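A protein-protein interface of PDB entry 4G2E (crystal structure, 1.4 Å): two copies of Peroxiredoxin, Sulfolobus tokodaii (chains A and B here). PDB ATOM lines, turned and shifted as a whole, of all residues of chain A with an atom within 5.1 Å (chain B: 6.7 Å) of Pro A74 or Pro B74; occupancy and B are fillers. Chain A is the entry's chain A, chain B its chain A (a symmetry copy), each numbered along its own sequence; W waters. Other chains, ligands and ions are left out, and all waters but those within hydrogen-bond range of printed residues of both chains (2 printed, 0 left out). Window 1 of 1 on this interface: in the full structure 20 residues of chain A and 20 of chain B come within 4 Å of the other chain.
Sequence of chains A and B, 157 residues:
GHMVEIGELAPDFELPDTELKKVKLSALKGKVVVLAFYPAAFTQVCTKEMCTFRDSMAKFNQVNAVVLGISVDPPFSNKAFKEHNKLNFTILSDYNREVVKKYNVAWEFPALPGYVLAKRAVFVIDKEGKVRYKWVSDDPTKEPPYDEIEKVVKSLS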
ATOM      1  N   VAL A  72      30.718   3.827  -8.332  1.00  0.00           N
ATOM      2  CA  VAL A  72      30.803   3.496  -9.752  1.00  0.00           C
ATOM      3  C   VAL A  72      29.433   3.278 -10.403  1.00  0.00           C
ATOM      4  O   VAL A  72      29.352   2.916 -11.571  1.00  0.00           O
ATOM      5  CB  VAL A  72      31.683   2.261 -10.012  1.00  0.00           C
ATOM      6  CG1 VAL A  72      33.083   2.462  -9.429  1.00  0.00           C
ATOM      7  CG2 VAL A  72      31.043   1.016  -9.441  1.00  0.00           C
ATOM      8  N   ASP A  73      28.364   3.494  -9.638  1.00  0.00           N
ATOM      9  CA  ASP A  73      27.021   3.416 -10.190  1.00  0.00           C
ATOM     10  C   ASP A  73      26.783   4.524 -11.197  1.00  0.00           C
ATOM     11  O   ASP A  73      27.362   5.593 -11.079  1.00  0.00           O
ATOM     12  CB  ASP A  73      26.007   3.553  -9.056  1.00  0.00           C
ATOM     13  CG  ASP A  73      26.224   2.509  -7.975  1.00  0.00           C
ATOM     14  OD1 ASP A  73      26.120   1.307  -8.288  1.00  0.00           O
ATOM     15  OD2 ASP A  73      26.535   2.885  -6.824  1.00  0.00           O
ATOM     16  N   PRO A  74      25.886   4.286 -12.174  1.00  0.00           N
ATOM     17  CA  PRO A  74      25.615   5.338 -13.162  1.00  0.00           C
ATOM     18  C   PRO A  74      24.799   6.475 -12.563  1.00  0.00           C
ATOM     19  O   PRO A  74      24.102   6.274 -11.558  1.00  0.00           O
ATOM     20  CB  PRO A  74      24.820   4.610 -14.237  1.00  0.00           C
ATOM     21  CG  PRO A  74      24.167   3.497 -13.532  1.00  0.00           C
ATOM     22  CD  PRO A  74      25.123   3.056 -12.453  1.00  0.00           C
ATOM     23  N   PRO A  75      24.847   7.665 -13.149  1.00  0.00           N
ATOM     24  CA  PRO A  75      24.223   8.841 -12.537  1.00  0.00           C
ATOM     25  C   PRO A  75      22.720   8.706 -12.357  1.00  0.00           C
ATOM     26  O   PRO A  75      22.189   9.220 -11.401  1.00  0.00           O
ATOM     27  CB  PRO A  75      24.526   9.961 -13.538  1.00  0.00           C
ATOM     28  CG  PRO A  75      25.777   9.517 -14.236  1.00  0.00           C
ATOM     29  CD  PRO A  75      25.620   8.016 -14.350  1.00  0.00           C
ATOM     30  N   PHE A  76      22.060   8.001 -13.265  1.00  0.00           N
ATOM     31  CA  PHE A  76      20.610   7.895 -13.228  1.00  0.00           C
ATOM     32  C   PHE A  76      20.186   7.116 -11.975  1.00  0.00           C
ATOM     33  O   PHE A  76      19.230   7.474 -11.294  1.00  0.00           O
ATOM     34  CB  PHE A  76      20.072   7.226 -14.510  1.00  0.00           C
ATOM     35  CG  PHE A  76      20.914   7.503 -15.755  1.00  0.00           C
ATOM     36  CD1 PHE A  76      20.809   8.704 -16.451  1.00  0.00           C
ATOM     37  CD2 PHE A  76      21.823   6.561 -16.207  1.00  0.00           C
ATOM     38  CE1 PHE A  76      21.581   8.934 -17.583  1.00  0.00           C
ATOM     39  CE2 PHE A  76      22.601   6.789 -17.324  1.00  0.00           C
ATOM     40  CZ  PHE A  76      22.489   7.982 -18.007  1.00  0.00           C
ATOM     41  N   SER A  77      20.908   6.048 -11.669  1.00  0.00           N
ATOM     42  CA  SER A  77      20.639   5.243 -10.476  1.00  0.00           C
ATOM     43  C   SER A  77      21.075   5.975  -9.221  1.00  0.00           C
ATOM     44  O   SER A  77      20.370   5.955  -8.197  1.00  0.00           O
ATOM     45  CB  SER A  77      21.337   3.885 -10.581  1.00  0.00           C
ATOM     46  OG  SER A  77      20.688   3.066 -11.535  1.00  0.00           O
ATOM     47  N   ASN A  78      22.224   6.639  -9.280  1.00  0.00           N
ATOM     48  CA  ASN A  78      22.641   7.430  -8.129  1.00  0.00           C
ATOM     49  C   ASN A  78      21.644   8.552  -7.822  1.00  0.00           C
ATOM     50  O   ASN A  78      21.453   8.911  -6.664  1.00  0.00           O
ATOM     51  CB  ASN A  78      24.052   7.981  -8.309  1.00  0.00           C
ATOM     52  CG  ASN A  78      25.102   7.096  -7.675  1.00  0.00           C
ATOM     53  OD1 ASN A  78      24.798   6.250  -6.840  1.00  0.00           O
ATOM     54  ND2 ASN A  78      26.350   7.293  -8.061  1.00  0.00           N
ATOM     55  N   LYS A  79      20.977   9.083  -8.843  1.00  0.00           N
ATOM     56  CA  LYS A  79      19.971  10.122  -8.608  1.00  0.00           C
ATOM     57  C   LYS A  79      18.803   9.541  -7.807  1.00  0.00           C
ATOM     58  O   LYS A  79      18.357  10.138  -6.833  1.00  0.00           O
ATOM     59  CB  LYS A  79      19.471  10.717  -9.930  1.00  0.00           C
ATOM     60  CG  LYS A  79      18.379  11.770  -9.758  1.00  0.00           C
ATOM     61  CD  LYS A  79      18.081  12.470 -11.074  1.00  0.00           C
ATOM     62  CE  LYS A  79      16.863  13.375 -10.958  1.00  0.00           C
ATOM     63  NZ  LYS A  79      16.831  14.424 -11.997  1.00  0.00           N
ATOM     64  N   SER A  93      29.358   9.899 -10.119  1.00  0.00           N
ATOM     65  CA  SER A  93      29.468   8.577 -10.725  1.00  0.00           C
ATOM     66  C   SER A  93      30.805   8.346 -11.423  1.00  0.00           C
ATOM     67  O   SER A  93      31.051   8.863 -12.509  1.00  0.00           O
ATOM     68  CB  SER A  93      28.356   8.359 -11.735  1.00  0.00           C
ATOM     69  OG  SER A  93      27.083   8.445 -11.133  1.00  0.00           O
ATOM     70  N   TYR A 115      33.749  -6.992 -11.948  1.00  0.00           N
ATOM     71  CA  TYR A 115      33.031  -5.785 -11.528  1.00  0.00           C
ATOM     72  C   TYR A 115      33.855  -5.041 -10.502  1.00  0.00           C
ATOM     73  O   TYR A 115      33.949  -5.474  -9.353  1.00  0.00           O
ATOM     74  CB  TYR A 115      31.657  -6.116 -10.923  1.00  0.00           C
ATOM     75  CG  TYR A 115      30.815  -4.876 -10.658  1.00  0.00           C
ATOM     76  CD1 TYR A 115      30.139  -4.251 -11.698  1.00  0.00           C
ATOM     77  CD2 TYR A 115      30.690  -4.325  -9.377  1.00  0.00           C
ATOM     78  CE1 TYR A 115      29.375  -3.114 -11.487  1.00  0.00           C
ATOM     79  CE2 TYR A 115      29.917  -3.175  -9.151  1.00  0.00           C
ATOM     80  CZ  TYR A 115      29.258  -2.584 -10.215  1.00  0.00           C
ATOM     81  OH  TYR A 115      28.510  -1.457 -10.036  1.00  0.00           O
ATOM     82  N   THR B  18      18.877  -9.667 -10.631  1.00  0.00           N
ATOM     83  CA  THR B  18      18.844  -8.706  -9.535  1.00  0.00           C
ATOM     84  C   THR B  18      19.178  -9.312  -8.161  1.00  0.00           C
ATOM     85  O   THR B  18      19.413  -8.565  -7.220  1.00  0.00           O
ATOM     86  CB  THR B  18      17.486  -7.978  -9.495  1.00  0.00           C
ATOM     87  OG1 THR B  18      16.414  -8.928  -9.529  1.00  0.00           O
ATOM     88  CG2 THR B  18      17.367  -7.064 -10.706  1.00  0.00           C
ATOM     89  N   ALA B  40      18.918   2.624 -19.507  1.00  0.00           N
ATOM     90  CA  ALA B  40      19.226   2.947 -18.126  1.00  0.00           C
ATOM     91  C   ALA B  40      18.041   2.871 -17.180  1.00  0.00           C
ATOM     92  O   ALA B  40      17.010   3.491 -17.396  1.00  0.00           O
ATOM     93  CB  ALA B  40      19.845   4.332 -18.032  1.00  0.00           C
ATOM     94  N   ALA B  41      18.229   2.128 -16.098  1.00  0.00           N
ATOM     95  CA  ALA B  41      17.297   2.161 -14.982  1.00  0.00           C
ATOM     96  C   ALA B  41      17.111   3.588 -14.494  1.00  0.00           C
ATOM     97  O   ALA B  41      18.062   4.370 -14.459  1.00  0.00           O
ATOM     98  CB  ALA B  41      17.826   1.305 -13.850  1.00  0.00           C
ATOM     99  N   SER B  71      20.105  -4.375 -19.087  1.00  0.00           N
ATOM    100  CA  SER B  71      20.773  -3.081 -19.170  1.00  0.00           C
ATOM    101  C   SER B  71      22.172  -3.216 -18.587  1.00  0.00           C
ATOM    102  O   SER B  71      22.492  -4.224 -17.958  1.00  0.00           O
ATOM    103  CB  SER B  71      20.007  -2.016 -18.391  1.00  0.00           C
ATOM    104  OG  SER B  71      20.211  -2.151 -16.993  1.00  0.00           O
ATOM    105  N   VAL B  72      22.987  -2.181 -18.759  1.00  0.00           N
ATOM    106  CA  VAL B  72      24.343  -2.183 -18.214  1.00  0.00           C
ATOM    107  C   VAL B  72      24.414  -1.665 -16.775  1.00  0.00           C
ATOM    108  O   VAL B  72      25.497  -1.535 -16.216  1.00  0.00           O
ATOM    109  CB  VAL B  72      25.323  -1.379 -19.086  1.00  0.00           C
ATOM    110  CG1 VAL B  72      25.326  -1.905 -20.523  1.00  0.00           C
ATOM    111  CG2 VAL B  72      24.981   0.093 -19.060  1.00  0.00           C
ATOM    112  N   ASP B  73      23.257  -1.365 -16.187  1.00  0.00           N
ATOM    113  CA  ASP B  73      23.211  -0.966 -14.789  1.00  0.00           C
ATOM    114  C   ASP B  73      23.614  -2.112 -13.882  1.00  0.00           C
ATOM    115  O   ASP B  73      23.400  -3.265 -14.222  1.00  0.00           O
ATOM    116  CB  ASP B  73      21.786  -0.538 -14.440  1.00  0.00           C
ATOM    117  CG  ASP B  73      21.290   0.570 -15.352  1.00  0.00           C
ATOM    118  OD1 ASP B  73      21.906   1.654 -15.350  1.00  0.00           O
ATOM    119  OD2 ASP B  73      20.310   0.349 -16.096  1.00  0.00           O
ATOM    120  N   PRO B  74      24.163  -1.793 -12.694  1.00  0.00           N
ATOM    121  CA  PRO B  74      24.555  -2.874 -11.779  1.00  0.00           C
ATOM    122  C   PRO B  74      23.342  -3.541 -11.145  1.00  0.00           C
ATOM    123  O   PRO B  74      22.266  -2.929 -11.072  1.00  0.00           O
ATOM    124  CB  PRO B  74      25.388  -2.155 -10.728  1.00  0.00           C
ATOM    125  CG  PRO B  74      24.883  -0.773 -10.728  1.00  0.00           C
ATOM    126  CD  PRO B  74      24.492  -0.463 -12.151  1.00  0.00           C
ATOM    127  N   PRO B  75      23.475  -4.773 -10.669  1.00  0.00           N
ATOM    128  CA  PRO B  75      22.317  -5.536 -10.198  1.00  0.00           C
ATOM    129  C   PRO B  75      21.598  -4.887  -9.026  1.00  0.00           C
ATOM    130  O   PRO B  75      20.399  -5.000  -8.930  1.00  0.00           O
ATOM    131  CB  PRO B  75      22.931  -6.869  -9.754  1.00  0.00           C
ATOM    132  CG  PRO B  75      24.178  -7.003 -10.575  1.00  0.00           C
ATOM    133  CD  PRO B  75      24.701  -5.586 -10.683  1.00  0.00           C
ATOM    134  N   PHE B  76      22.336  -4.200  -8.166  1.00  0.00           N
ATOM    135  CA  PHE B  76      21.751  -3.622  -6.966  1.00  0.00           C
ATOM    136  C   PHE B  76      20.762  -2.516  -7.360  1.00  0.00           C
ATOM    137  O   PHE B  76      19.677  -2.402  -6.799  1.00  0.00           O
ATOM    138  CB  PHE B  76      22.846  -3.083  -6.022  1.00  0.00           C
ATOM    139  CG  PHE B  76      24.161  -3.859  -6.089  1.00  0.00           C
ATOM    140  CD1 PHE B  76      24.323  -5.073  -5.427  1.00  0.00           C
ATOM    141  CD2 PHE B  76      25.222  -3.373  -6.835  1.00  0.00           C
ATOM    142  CE1 PHE B  76      25.527  -5.761  -5.497  1.00  0.00           C
ATOM    143  CE2 PHE B  76      26.417  -4.058  -6.918  1.00  0.00           C
ATOM    144  CZ  PHE B  76      26.567  -5.260  -6.257  1.00  0.00           C
ATOM    145  N   SER B  77      21.141  -1.703  -8.335  1.00  0.00           N
ATOM    146  CA  SER B  77      20.275  -0.636  -8.838  1.00  0.00           C
ATOM    147  C   SER B  77      19.140  -1.205  -9.668  1.00  0.00           C
ATOM    148  O   SER B  77      17.986  -0.756  -9.562  1.00  0.00           O
ATOM    149  CB  SER B  77      21.089   0.372  -9.652  1.00  0.00           C
ATOM    150  OG  SER B  77      21.907   1.152  -8.801  1.00  0.00           O
ATOM    151  N   ASN B  78      19.441  -2.205 -10.490  1.00  0.00           N
ATOM    152  CA  ASN B  78      18.369  -2.845 -11.243  1.00  0.00           C
ATOM    153  C   ASN B  78      17.337  -3.497 -10.317  1.00  0.00           C
ATOM    154  O   ASN B  78      16.154  -3.538 -10.638  1.00  0.00           O
ATOM    155  CB  ASN B  78      18.915  -3.849 -12.253  1.00  0.00           C
ATOM    156  CG  ASN B  78      19.086  -3.246 -13.630  1.00  0.00           C
ATOM    157  OD1 ASN B  78      18.525  -2.201 -13.939  1.00  0.00           O
ATOM    158  ND2 ASN B  78      19.858  -3.911 -14.472  1.00  0.00           N
ATOM    159  N   LYS B  79      17.767  -3.973  -9.151  1.00  0.00           N
ATOM    160  CA  LYS B  79      16.820  -4.561  -8.199  1.00  0.00           C
ATOM    161  C   LYS B  79      15.852  -3.484  -7.701  1.00  0.00           C
ATOM    162  O   LYS B  79      14.645  -3.698  -7.670  1.00  0.00           O
ATOM    163  CB  LYS B  79      17.554  -5.209  -7.019  1.00  0.00           C
ATOM    164  CG  LYS B  79      16.621  -5.793  -5.960  1.00  0.00           C
ATOM    165  CD  LYS B  79      17.398  -6.604  -4.935  1.00  0.00           C
ATOM    166  CE  LYS B  79      16.510  -7.022  -3.771  1.00  0.00           C
ATOM    167  NZ  LYS B  79      17.044  -8.187  -3.037  1.00  0.00           N
ATOM    168  N   SER B  93      21.987  -7.707 -15.537  1.00  0.00           N
ATOM    169  CA  SER B  93      22.980  -6.640 -15.601  1.00  0.00           C
ATOM    170  C   SER B  93      24.193  -7.000 -16.454  1.00  0.00           C
ATOM    171  O   SER B  93      25.053  -7.772 -16.041  1.00  0.00           O
ATOM    172  CB  SER B  93      23.463  -6.276 -14.210  1.00  0.00           C
ATOM    173  OG  SER B  93      22.405  -5.822 -13.394  1.00  0.00           O
ATOM    174  N   TYR B  95      27.004  -5.799 -17.035  1.00  0.00           N
ATOM    175  CA  TYR B  95      27.863  -4.768 -16.465  1.00  0.00           C
ATOM    176  C   TYR B  95      29.208  -4.611 -17.196  1.00  0.00           C
ATOM    177  O   TYR B  95      29.834  -3.549 -17.124  1.00  0.00           O
ATOM    178  CB  TYR B  95      28.073  -4.993 -14.971  1.00  0.00           C
ATOM    179  CG  TYR B  95      28.715  -6.320 -14.613  1.00  0.00           C
ATOM    180  CD1 TYR B  95      30.092  -6.465 -14.590  1.00  0.00           C
ATOM    181  CD2 TYR B  95      27.942  -7.427 -14.309  1.00  0.00           C
ATOM    182  CE1 TYR B  95      30.687  -7.672 -14.245  1.00  0.00           C
ATOM    183  CE2 TYR B  95      28.527  -8.626 -13.969  1.00  0.00           C
ATOM    184  CZ  TYR B  95      29.900  -8.748 -13.950  1.00  0.00           C
ATOM    185  OH  TYR B  95      30.448  -9.958 -13.598  1.00  0.00           O
ATOM    186  N   LEU B 112      27.826  11.418 -21.497  1.00  0.00           N
ATOM    187  CA  LEU B 112      28.803  10.722 -20.666  1.00  0.00           C
ATOM    188  C   LEU B 112      29.877  10.049 -21.532  1.00  0.00           C
ATOM    189  O   LEU B 112      29.729   8.896 -21.942  1.00  0.00           O
ATOM    190  CB  LEU B 112      28.100   9.657 -19.816  1.00  0.00           C
ATOM    191  CG  LEU B 112      27.080  10.144 -18.777  1.00  0.00           C
ATOM    192  CD1 LEU B 112      26.311   8.966 -18.195  1.00  0.00           C
ATOM    193  CD2 LEU B 112      27.749  10.959 -17.664  1.00  0.00           C
ATOM    194  N   TYR B 115      30.825   6.122 -21.751  1.00  0.00           N
ATOM    195  CA  TYR B 115      29.782   5.322 -21.101  1.00  0.00           C
ATOM    196  C   TYR B 115      28.997   4.569 -22.150  1.00  0.00           C
ATOM    197  O   TYR B 115      28.194   5.166 -22.868  1.00  0.00           O
ATOM    198  CB  TYR B 115      28.816   6.195 -20.283  1.00  0.00           C
ATOM    199  CG  TYR B 115      27.846   5.375 -19.446  1.00  0.00           C
ATOM    200  CD1 TYR B 115      28.257   4.811 -18.245  1.00  0.00           C
ATOM    201  CD2 TYR B 115      26.521   5.160 -19.845  1.00  0.00           C
ATOM    202  CE1 TYR B 115      27.397   4.050 -17.468  1.00  0.00           C
ATOM    203  CE2 TYR B 115      25.640   4.392 -19.067  1.00  0.00           C
ATOM    204  CZ  TYR B 115      26.090   3.850 -17.875  1.00  0.00           C
ATOM    205  OH  TYR B 115      25.267   3.086 -17.099  1.00  0.00           O
HETATM  206  O   HOH W   1      20.805   3.855 -14.123  1.00  0.00           O
HETATM  207  O   HOH W   2      23.909  -0.128  -7.502  1.00  0.00           O
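Of chain B, only Asp B73, Pro B74 and Tyr B115 come within 4 Å of Pro A74.
Printed residues of chain A within 4 Å of Ala B40: Phe A76.
Pro B74 touches just these residues of chain A: Asp A73 (3.4 Å), Pro A74 (3.6 Å) and Tyr A115 (3.3 Å).
Of the printed residues of chain A, Leu B112 touches Phe A76 (3.95 Å).
The nearest residue of chain B that does not touch Pro A74 is Ser B77 (5.2 Å).
The nearest printed residue of chain B that does not touch Ser A77 is Ala B41 (4.1 Å).
The backbone carbonyl oxygen of Asp A73 lies within hydrogen-bond range of the side-chain hydroxyl of Ser A93 (2.9 Å).
OD2 of Asp B73 is in hydrogen-bond range of N of Ala B41 (2.7 Å).
The side-chain carboxylate of Asp B73 sits at hydrogen-bond distance from the side-chain hydroxyl of Ser B71, at 2.7 Å.
The backbone carbonyl oxygen (O) of Asp B73 is in hydrogen-bond range of the side-chain hydroxyl (OG) of Ser B93 (2.9 Å).
Water W2 bridges OG of Ser B77 (2.7 Å) and OD1 of Asp A73 (2.8 Å).
Water W1 lies within hydrogen-bond range of the side-chain hydroxyl of Ser A77, the side-chain carboxylate of Asp B73 and the backbone carbonyl oxygen of Ala B41.
Among the printed residues, pairs that only touch across the chains: Tyr A115 with Pro B74 (3.3 Å), Pro A74 with Tyr B115 (3.3 Å), Ser A77 with Ser B77 (3.3 Å), Asp A73 with Pro B74 (3.4 Å), Pro A74 with Asp B73 (3.4 Å), Phe A76 with Ala B41 (3.5 Å), Phe A76 with Ala B40 (3.5 Å), Pro A74 with Pro B74 (3.6 Å), Tyr A115 with Tyr B95 (3.6 Å) and Phe A76 with Leu B112 (3.95 Å).
Asp A73 touches Pro B74, and with the chains exchanged Pro A74 touches Asp B73.
Pro B74 touches its own counterpart, Pro A74.
Pro A74 touches Tyr B115, and with the chains exchanged Tyr A115 touches Pro B74.
Ser B77 touches its own counterpart, Ser A77.
Of the 10 pairs that touch across the chains among the printed residues, 6 have their exchanged pair printed and touching as well.
Of the 16 printed residues of chain B, 8 touch a printed residue of chain A.
Hydrophobic or aromatic side chains of chain B within 4 Å of the printed part of chain A: Ala B40, Pro B74, Tyr B95, Leu B112 and Tyr B115.
Hydrophobic or aromatic side chains of chain A that line the printed part of chain B: Pro A74, Phe A76 and Tyr A115.
Among the printed residues, 10 pairs touch across the chains.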
